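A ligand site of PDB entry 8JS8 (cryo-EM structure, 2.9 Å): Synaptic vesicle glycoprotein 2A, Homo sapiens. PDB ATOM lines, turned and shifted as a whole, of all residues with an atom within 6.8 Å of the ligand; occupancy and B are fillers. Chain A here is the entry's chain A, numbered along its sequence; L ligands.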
ATOM      1  N   LEU A 184      26.330  14.772 -17.940  1.00  0.00           N
ATOM      2  CA  LEU A 184      25.394  13.661 -18.071  1.00  0.00           C
ATOM      3  C   LEU A 184      24.185  13.786 -17.154  1.00  0.00           C
ATOM      4  O   LEU A 184      23.091  13.334 -17.507  1.00  0.00           O
ATOM      5  CB  LEU A 184      26.109  12.330 -17.762  1.00  0.00           C
ATOM      6  CG  LEU A 184      25.917  11.183 -18.736  1.00  0.00           C
ATOM      7  CD1 LEU A 184      26.325  11.589 -20.137  1.00  0.00           C
ATOM      8  CD2 LEU A 184      26.725   9.986 -18.273  1.00  0.00           C
ATOM      9  N   ASP A 187      21.469  15.670 -18.906  1.00  0.00           N
ATOM     10  CA  ASP A 187      20.667  14.806 -19.758  1.00  0.00           C
ATOM     11  C   ASP A 187      19.708  13.942 -18.945  1.00  0.00           C
ATOM     12  O   ASP A 187      18.564  13.732 -19.339  1.00  0.00           O
ATOM     13  CB  ASP A 187      21.578  13.931 -20.618  1.00  0.00           C
ATOM     14  CG  ASP A 187      20.853  13.260 -21.775  1.00  0.00           C
ATOM     15  OD1 ASP A 187      19.881  12.516 -21.521  1.00  0.00           O
ATOM     16  OD2 ASP A 187      21.256  13.462 -22.932  1.00  0.00           O
ATOM     17  N   ILE A 281      25.363  12.553 -24.285  1.00  0.00           N
ATOM     18  CA  ILE A 281      25.907  11.219 -23.980  1.00  0.00           C
ATOM     19  C   ILE A 281      27.027  10.805 -24.937  1.00  0.00           C
ATOM     20  O   ILE A 281      28.101  10.405 -24.456  1.00  0.00           O
ATOM     21  CB  ILE A 281      24.765  10.181 -23.929  1.00  0.00           C
ATOM     22  CG1 ILE A 281      23.877  10.438 -22.715  1.00  0.00           C
ATOM     23  CG2 ILE A 281      25.313   8.773 -23.906  1.00  0.00           C
ATOM     24  CD1 ILE A 281      22.696   9.508 -22.631  1.00  0.00           C
ATOM     25  N   PHE A 285      30.879  10.423 -23.404  1.00  0.00           N
ATOM     26  CA  PHE A 285      31.538   9.121 -23.305  1.00  0.00           C
ATOM     27  C   PHE A 285      32.796   9.059 -24.175  1.00  0.00           C
ATOM     28  O   PHE A 285      33.850   8.592 -23.727  1.00  0.00           O
ATOM     29  CB  PHE A 285      30.561   8.001 -23.654  1.00  0.00           C
ATOM     30  CG  PHE A 285      29.730   7.545 -22.494  1.00  0.00           C
ATOM     31  CD1 PHE A 285      30.299   6.786 -21.485  1.00  0.00           C
ATOM     32  CD2 PHE A 285      28.398   7.874 -22.405  1.00  0.00           C
ATOM     33  CE1 PHE A 285      29.547   6.373 -20.406  1.00  0.00           C
ATOM     34  CE2 PHE A 285      27.642   7.453 -21.326  1.00  0.00           C
ATOM     35  CZ  PHE A 285      28.217   6.702 -20.326  1.00  0.00           C
ATOM     36  N   LEU A 304      30.795   6.255 -14.822  1.00  0.00           N
ATOM     37  CA  LEU A 304      30.265   7.505 -15.356  1.00  0.00           C
ATOM     38  C   LEU A 304      28.743   7.495 -15.492  1.00  0.00           C
ATOM     39  O   LEU A 304      28.161   8.552 -15.749  1.00  0.00           O
ATOM     40  CB  LEU A 304      30.896   7.806 -16.714  1.00  0.00           C
ATOM     41  CG  LEU A 304      30.926   9.241 -17.231  1.00  0.00           C
ATOM     42  CD1 LEU A 304      31.602  10.161 -16.247  1.00  0.00           C
ATOM     43  CD2 LEU A 304      31.611   9.299 -18.579  1.00  0.00           C
ATOM     44  N   CYS A 305      28.096   6.352 -15.309  1.00  0.00           N
ATOM     45  CA  CYS A 305      26.644   6.251 -15.464  1.00  0.00           C
ATOM     46  C   CYS A 305      25.895   6.454 -14.149  1.00  0.00           C
ATOM     47  O   CYS A 305      24.668   6.351 -14.141  1.00  0.00           O
ATOM     48  CB  CYS A 305      26.274   4.892 -16.067  1.00  0.00           C
ATOM     49  SG  CYS A 305      27.037   4.566 -17.672  1.00  0.00           S
ATOM     50  N   TRP A 308      23.672   9.889 -14.303  1.00  0.00           N
ATOM     51  CA  TRP A 308      22.342   9.853 -14.897  1.00  0.00           C
ATOM     52  C   TRP A 308      21.276   9.525 -13.853  1.00  0.00           C
ATOM     53  O   TRP A 308      20.232  10.181 -13.787  1.00  0.00           O
ATOM     54  CB  TRP A 308      22.330   8.850 -16.049  1.00  0.00           C
ATOM     55  CG  TRP A 308      21.107   8.842 -16.880  1.00  0.00           C
ATOM     56  CD1 TRP A 308      20.827   9.659 -17.939  1.00  0.00           C
ATOM     57  CD2 TRP A 308      20.005   7.938 -16.774  1.00  0.00           C
ATOM     58  NE1 TRP A 308      19.602   9.341 -18.474  1.00  0.00           N
ATOM     59  CE2 TRP A 308      19.082   8.282 -17.778  1.00  0.00           C
ATOM     60  CE3 TRP A 308      19.698   6.872 -15.927  1.00  0.00           C
ATOM     61  CZ2 TRP A 308      17.878   7.605 -17.952  1.00  0.00           C
ATOM     62  CZ3 TRP A 308      18.507   6.199 -16.099  1.00  0.00           C
ATOM     63  CH2 TRP A 308      17.607   6.565 -17.100  1.00  0.00           C
ATOM     64  N   TRP A 462      21.221  -1.418 -30.121  1.00  0.00           N
ATOM     65  CA  TRP A 462      20.752  -0.128 -29.627  1.00  0.00           C
ATOM     66  C   TRP A 462      19.244   0.005 -29.813  1.00  0.00           C
ATOM     67  O   TRP A 462      18.519   0.364 -28.880  1.00  0.00           O
ATOM     68  CB  TRP A 462      21.476   1.009 -30.355  1.00  0.00           C
ATOM     69  CG  TRP A 462      22.794   1.398 -29.737  1.00  0.00           C
ATOM     70  CD1 TRP A 462      24.028   0.956 -30.101  1.00  0.00           C
ATOM     71  CD2 TRP A 462      22.998   2.331 -28.678  1.00  0.00           C
ATOM     72  NE1 TRP A 462      24.991   1.540 -29.324  1.00  0.00           N
ATOM     73  CE2 TRP A 462      24.384   2.393 -28.441  1.00  0.00           C
ATOM     74  CE3 TRP A 462      22.142   3.116 -27.890  1.00  0.00           C
ATOM     75  CZ2 TRP A 462      24.931   3.199 -27.453  1.00  0.00           C
ATOM     76  CZ3 TRP A 462      22.699   3.917 -26.910  1.00  0.00           C
ATOM     77  CH2 TRP A 462      24.076   3.953 -26.704  1.00  0.00           C
ATOM     78  N   SER A 466      16.682   0.085 -26.604  1.00  0.00           N
ATOM     79  CA  SER A 466      15.997   1.359 -26.403  1.00  0.00           C
ATOM     80  C   SER A 466      14.487   1.183 -26.505  1.00  0.00           C
ATOM     81  O   SER A 466      13.728   1.690 -25.669  1.00  0.00           O
ATOM     82  CB  SER A 466      16.491   2.384 -27.425  1.00  0.00           C
ATOM     83  OG  SER A 466      17.906   2.435 -27.426  1.00  0.00           O
ATOM     84  N   TYR A 469      13.222  -0.773 -23.339  1.00  0.00           N
ATOM     85  CA  TYR A 469      13.381  -0.008 -22.103  1.00  0.00           C
ATOM     86  C   TYR A 469      12.395   1.148 -22.045  1.00  0.00           C
ATOM     87  O   TYR A 469      11.685   1.315 -21.047  1.00  0.00           O
ATOM     88  CB  TYR A 469      14.817   0.509 -21.985  1.00  0.00           C
ATOM     89  CG  TYR A 469      15.024   1.434 -20.814  1.00  0.00           C
ATOM     90  CD1 TYR A 469      15.269   0.937 -19.541  1.00  0.00           C
ATOM     91  CD2 TYR A 469      14.984   2.815 -20.977  1.00  0.00           C
ATOM     92  CE1 TYR A 469      15.462   1.785 -18.473  1.00  0.00           C
ATOM     93  CE2 TYR A 469      15.170   3.668 -19.920  1.00  0.00           C
ATOM     94  CZ  TYR A 469      15.409   3.152 -18.668  1.00  0.00           C
ATOM     95  OH  TYR A 469      15.602   4.000 -17.599  1.00  0.00           O
ATOM     96  N   TYR A 470      12.340   1.962 -23.102  1.00  0.00           N
ATOM     97  CA  TYR A 470      11.460   3.120 -23.069  1.00  0.00           C
ATOM     98  C   TYR A 470       9.997   2.712 -23.081  1.00  0.00           C
ATOM     99  O   TYR A 470       9.163   3.334 -22.399  1.00  0.00           O
ATOM    100  CB  TYR A 470      11.791   4.057 -24.225  1.00  0.00           C
ATOM    101  CG  TYR A 470      13.051   4.860 -23.984  1.00  0.00           C
ATOM    102  CD1 TYR A 470      13.038   5.950 -23.129  1.00  0.00           C
ATOM    103  CD2 TYR A 470      14.247   4.519 -24.577  1.00  0.00           C
ATOM    104  CE1 TYR A 470      14.184   6.687 -22.893  1.00  0.00           C
ATOM    105  CE2 TYR A 470      15.399   5.242 -24.350  1.00  0.00           C
ATOM    106  CZ  TYR A 470      15.361   6.324 -23.509  1.00  0.00           C
ATOM    107  OH  TYR A 470      16.502   7.052 -23.274  1.00  0.00           O
ATOM    108  N   VAL A 616      18.160   1.578 -10.014  1.00  0.00           N
ATOM    109  CA  VAL A 616      19.341   1.553 -10.856  1.00  0.00           C
ATOM    110  C   VAL A 616      20.607   1.403 -10.017  1.00  0.00           C
ATOM    111  O   VAL A 616      21.590   0.790 -10.446  1.00  0.00           O
ATOM    112  CB  VAL A 616      19.381   2.814 -11.743  1.00  0.00           C
ATOM    113  CG1 VAL A 616      20.788   3.206 -12.103  1.00  0.00           C
ATOM    114  CG2 VAL A 616      18.555   2.596 -13.000  1.00  0.00           C
ATOM    115  N   SER A 670      18.149  -3.787 -16.006  1.00  0.00           N
ATOM    116  CA  SER A 670      18.607  -3.377 -17.339  1.00  0.00           C
ATOM    117  C   SER A 670      19.796  -2.423 -17.322  1.00  0.00           C
ATOM    118  O   SER A 670      20.403  -2.174 -18.390  1.00  0.00           O
ATOM    119  CB  SER A 670      17.446  -2.723 -18.108  1.00  0.00           C
ATOM    120  OG  SER A 670      16.547  -3.707 -18.579  1.00  0.00           O
ATOM    121  N   ILE A 671      20.162  -1.872 -16.165  1.00  0.00           N
ATOM    122  CA  ILE A 671      21.179  -0.831 -16.133  1.00  0.00           C
ATOM    123  C   ILE A 671      22.556  -1.405 -16.465  1.00  0.00           C
ATOM    124  O   ILE A 671      23.395  -0.738 -17.091  1.00  0.00           O
ATOM    125  CB  ILE A 671      21.164  -0.085 -14.790  1.00  0.00           C
ATOM    126  CG1 ILE A 671      21.960   1.213 -14.893  1.00  0.00           C
ATOM    127  CG2 ILE A 671      21.688  -0.963 -13.665  1.00  0.00           C
ATOM    128  CD1 ILE A 671      21.410   2.178 -15.922  1.00  0.00           C
ATOM    129  N   TRP A 674      22.810  -1.635 -20.134  1.00  0.00           N
ATOM    130  CA  TRP A 674      23.022  -0.311 -20.735  1.00  0.00           C
ATOM    131  C   TRP A 674      24.472   0.139 -20.563  1.00  0.00           C
ATOM    132  O   TRP A 674      25.070   0.690 -21.505  1.00  0.00           O
ATOM    133  CB  TRP A 674      22.059   0.698 -20.126  1.00  0.00           C
ATOM    134  CG  TRP A 674      20.731   0.688 -20.800  1.00  0.00           C
ATOM    135  CD1 TRP A 674      19.592   0.097 -20.340  1.00  0.00           C
ATOM    136  CD2 TRP A 674      20.400   1.263 -22.066  1.00  0.00           C
ATOM    137  NE1 TRP A 674      18.570   0.282 -21.235  1.00  0.00           N
ATOM    138  CE2 TRP A 674      19.044   0.994 -22.307  1.00  0.00           C
ATOM    139  CE3 TRP A 674      21.120   1.977 -23.022  1.00  0.00           C
ATOM    140  CZ2 TRP A 674      18.393   1.423 -23.465  1.00  0.00           C
ATOM    141  CZ3 TRP A 674      20.476   2.401 -24.169  1.00  0.00           C
ATOM    142  CH2 TRP A 674      19.125   2.128 -24.379  1.00  0.00           C
ATOM    143  N   ASN A 675      25.051  -0.095 -19.387  1.00  0.00           N
ATOM    144  CA  ASN A 675      26.469   0.222 -19.168  1.00  0.00           C
ATOM    145  C   ASN A 675      27.353  -0.543 -20.145  1.00  0.00           C
ATOM    146  O   ASN A 675      28.293   0.024 -20.724  1.00  0.00           O
ATOM    147  CB  ASN A 675      26.860  -0.124 -17.725  1.00  0.00           C
ATOM    148  CG  ASN A 675      26.319   0.868 -16.722  1.00  0.00           C
ATOM    149  OD1 ASN A 675      27.033   1.757 -16.267  1.00  0.00           O
ATOM    150  ND2 ASN A 675      25.046   0.711 -16.367  1.00  0.00           N
ATOM    151  N   LEU A 677      26.583  -1.767 -23.089  1.00  0.00           N
ATOM    152  CA  LEU A 677      26.430  -1.245 -24.440  1.00  0.00           C
ATOM    153  C   LEU A 677      27.186   0.066 -24.610  1.00  0.00           C
ATOM    154  O   LEU A 677      27.820   0.289 -25.644  1.00  0.00           O
ATOM    155  CB  LEU A 677      24.959  -1.065 -24.784  1.00  0.00           C
ATOM    156  CG  LEU A 677      24.704  -0.489 -26.170  1.00  0.00           C
ATOM    157  CD1 LEU A 677      25.245  -1.432 -27.234  1.00  0.00           C
ATOM    158  CD2 LEU A 677      23.233  -0.228 -26.383  1.00  0.00           C
ATOM    159  N   ASP A 678      27.144   0.949 -23.606  1.00  0.00           N
ATOM    160  CA  ASP A 678      27.898   2.198 -23.674  1.00  0.00           C
ATOM    161  C   ASP A 678      29.387   1.929 -23.843  1.00  0.00           C
ATOM    162  O   ASP A 678      30.041   2.492 -24.736  1.00  0.00           O
ATOM    163  CB  ASP A 678      27.641   3.041 -22.428  1.00  0.00           C
ATOM    164  CG  ASP A 678      26.281   3.705 -22.427  1.00  0.00           C
ATOM    165  OD1 ASP A 678      25.735   3.940 -23.518  1.00  0.00           O
ATOM    166  OD2 ASP A 678      25.771   4.000 -21.331  1.00  0.00           O
ATOM    167  N   PHE A 694      28.663   7.062 -32.409  1.00  0.00           N
ATOM    168  CA  PHE A 694      27.915   7.075 -31.152  1.00  0.00           C
ATOM    169  C   PHE A 694      26.669   7.947 -31.269  1.00  0.00           C
ATOM    170  O   PHE A 694      25.590   7.560 -30.803  1.00  0.00           O
ATOM    171  CB  PHE A 694      28.817   7.556 -30.019  1.00  0.00           C
ATOM    172  CG  PHE A 694      28.457   6.992 -28.660  1.00  0.00           C
ATOM    173  CD1 PHE A 694      27.150   6.719 -28.328  1.00  0.00           C
ATOM    174  CD2 PHE A 694      29.450   6.740 -27.727  1.00  0.00           C
ATOM    175  CE1 PHE A 694      26.826   6.212 -27.085  1.00  0.00           C
ATOM    176  CE2 PHE A 694      29.134   6.229 -26.484  1.00  0.00           C
ATOM    177  CZ  PHE A 694      27.825   5.969 -26.162  1.00  0.00           C
ATOM    178  N   ASN A 698      22.816   6.860 -31.059  1.00  0.00           N
ATOM    179  CA  ASN A 698      21.963   7.495 -30.056  1.00  0.00           C
ATOM    180  C   ASN A 698      20.706   8.089 -30.687  1.00  0.00           C
ATOM    181  O   ASN A 698      19.634   8.061 -30.082  1.00  0.00           O
ATOM    182  CB  ASN A 698      22.750   8.564 -29.300  1.00  0.00           C
ATOM    183  CG  ASN A 698      22.536   8.491 -27.804  1.00  0.00           C
ATOM    184  OD1 ASN A 698      22.568   7.414 -27.211  1.00  0.00           O
ATOM    185  ND2 ASN A 698      22.319   9.645 -27.191  1.00  0.00           N
ATOM    186  N   CYS A 701      18.554   5.267 -31.103  1.00  0.00           N
ATOM    187  CA  CYS A 701      17.983   4.961 -29.787  1.00  0.00           C
ATOM    188  C   CYS A 701      16.786   5.849 -29.483  1.00  0.00           C
ATOM    189  O   CYS A 701      15.762   5.386 -28.967  1.00  0.00           O
ATOM    190  CB  CYS A 701      19.056   5.121 -28.716  1.00  0.00           C
ATOM    191  SG  CYS A 701      18.436   5.325 -27.039  1.00  0.00           S
ATOM    192  N   LYS A 702      16.897   7.151 -29.795  1.00  0.00           N
ATOM    193  CA  LYS A 702      15.787   8.064 -29.529  1.00  0.00           C
ATOM    194  C   LYS A 702      14.599   7.796 -30.443  1.00  0.00           C
ATOM    195  O   LYS A 702      13.442   7.902 -30.014  1.00  0.00           O
ATOM    196  CB  LYS A 702      16.265   9.505 -29.670  1.00  0.00           C
ATOM    197  CG  LYS A 702      17.330   9.910 -28.674  1.00  0.00           C
ATOM    198  CD  LYS A 702      16.966   9.437 -27.276  1.00  0.00           C
ATOM    199  CE  LYS A 702      18.085   9.725 -26.291  1.00  0.00           C
ATOM    200  NZ  LYS A 702      17.809   9.142 -24.950  1.00  0.00           N
HETATM  201  O1  LIG L   1      19.318   6.033 -22.143  1.00  0.00           O
HETATM  202  O2  LIG L   1      23.102   4.182 -21.795  1.00  0.00           O
HETATM  203  N1  LIG L   1      20.760   5.401 -20.436  1.00  0.00           N
HETATM  204  C1  LIG L   1      19.538   5.417 -21.115  1.00  0.00           C
HETATM  205  C2  LIG L   1      18.547   4.553 -20.388  1.00  0.00           C
HETATM  206  C3  LIG L   1      19.226   4.081 -19.114  1.00  0.00           C
HETATM  207  C4  LIG L   1      20.695   4.550 -19.233  1.00  0.00           C
HETATM  208  C5  LIG L   1      22.652   5.301 -21.953  1.00  0.00           C
HETATM  209  C6  LIG L   1      21.982   6.104 -20.825  1.00  0.00           C
HETATM  210  C7  LIG L   1      22.986   6.203 -19.653  1.00  0.00           C
HETATM  211  C8  LIG L   1      23.816   7.479 -19.680  1.00  0.00           C
HETATM  212  N2  LIG L   1      22.735   5.888 -23.210  1.00  0.00           N
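OD2 of Asp 678 lies close to O2 of the ligand (2.7 Å).
O1 of the ligand sits at hydrogen-bond distance from OH of Tyr 470.
The side-chain hydroxyl (OH) of Tyr 470 lies within hydrogen-bond range of the side-chain amino group (NZ) of Lys 702.
Merely in contact with the ligand: Ile 281 (3.7 Å), Trp 308 (3.6 Å), Tyr 469 (3.5 Å) and Trp 674 (3.2 Å).
Hydrophobic or aromatic side chains within 4 Å of the ligand: Ile 281, Trp 308, Tyr 469 and Trp 674.
Along chain A the residues within 4 Å of the ligand span positions 281 to 678.
The nearest printed residue that does not touch the ligand is Leu 184 (4.1 Å).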
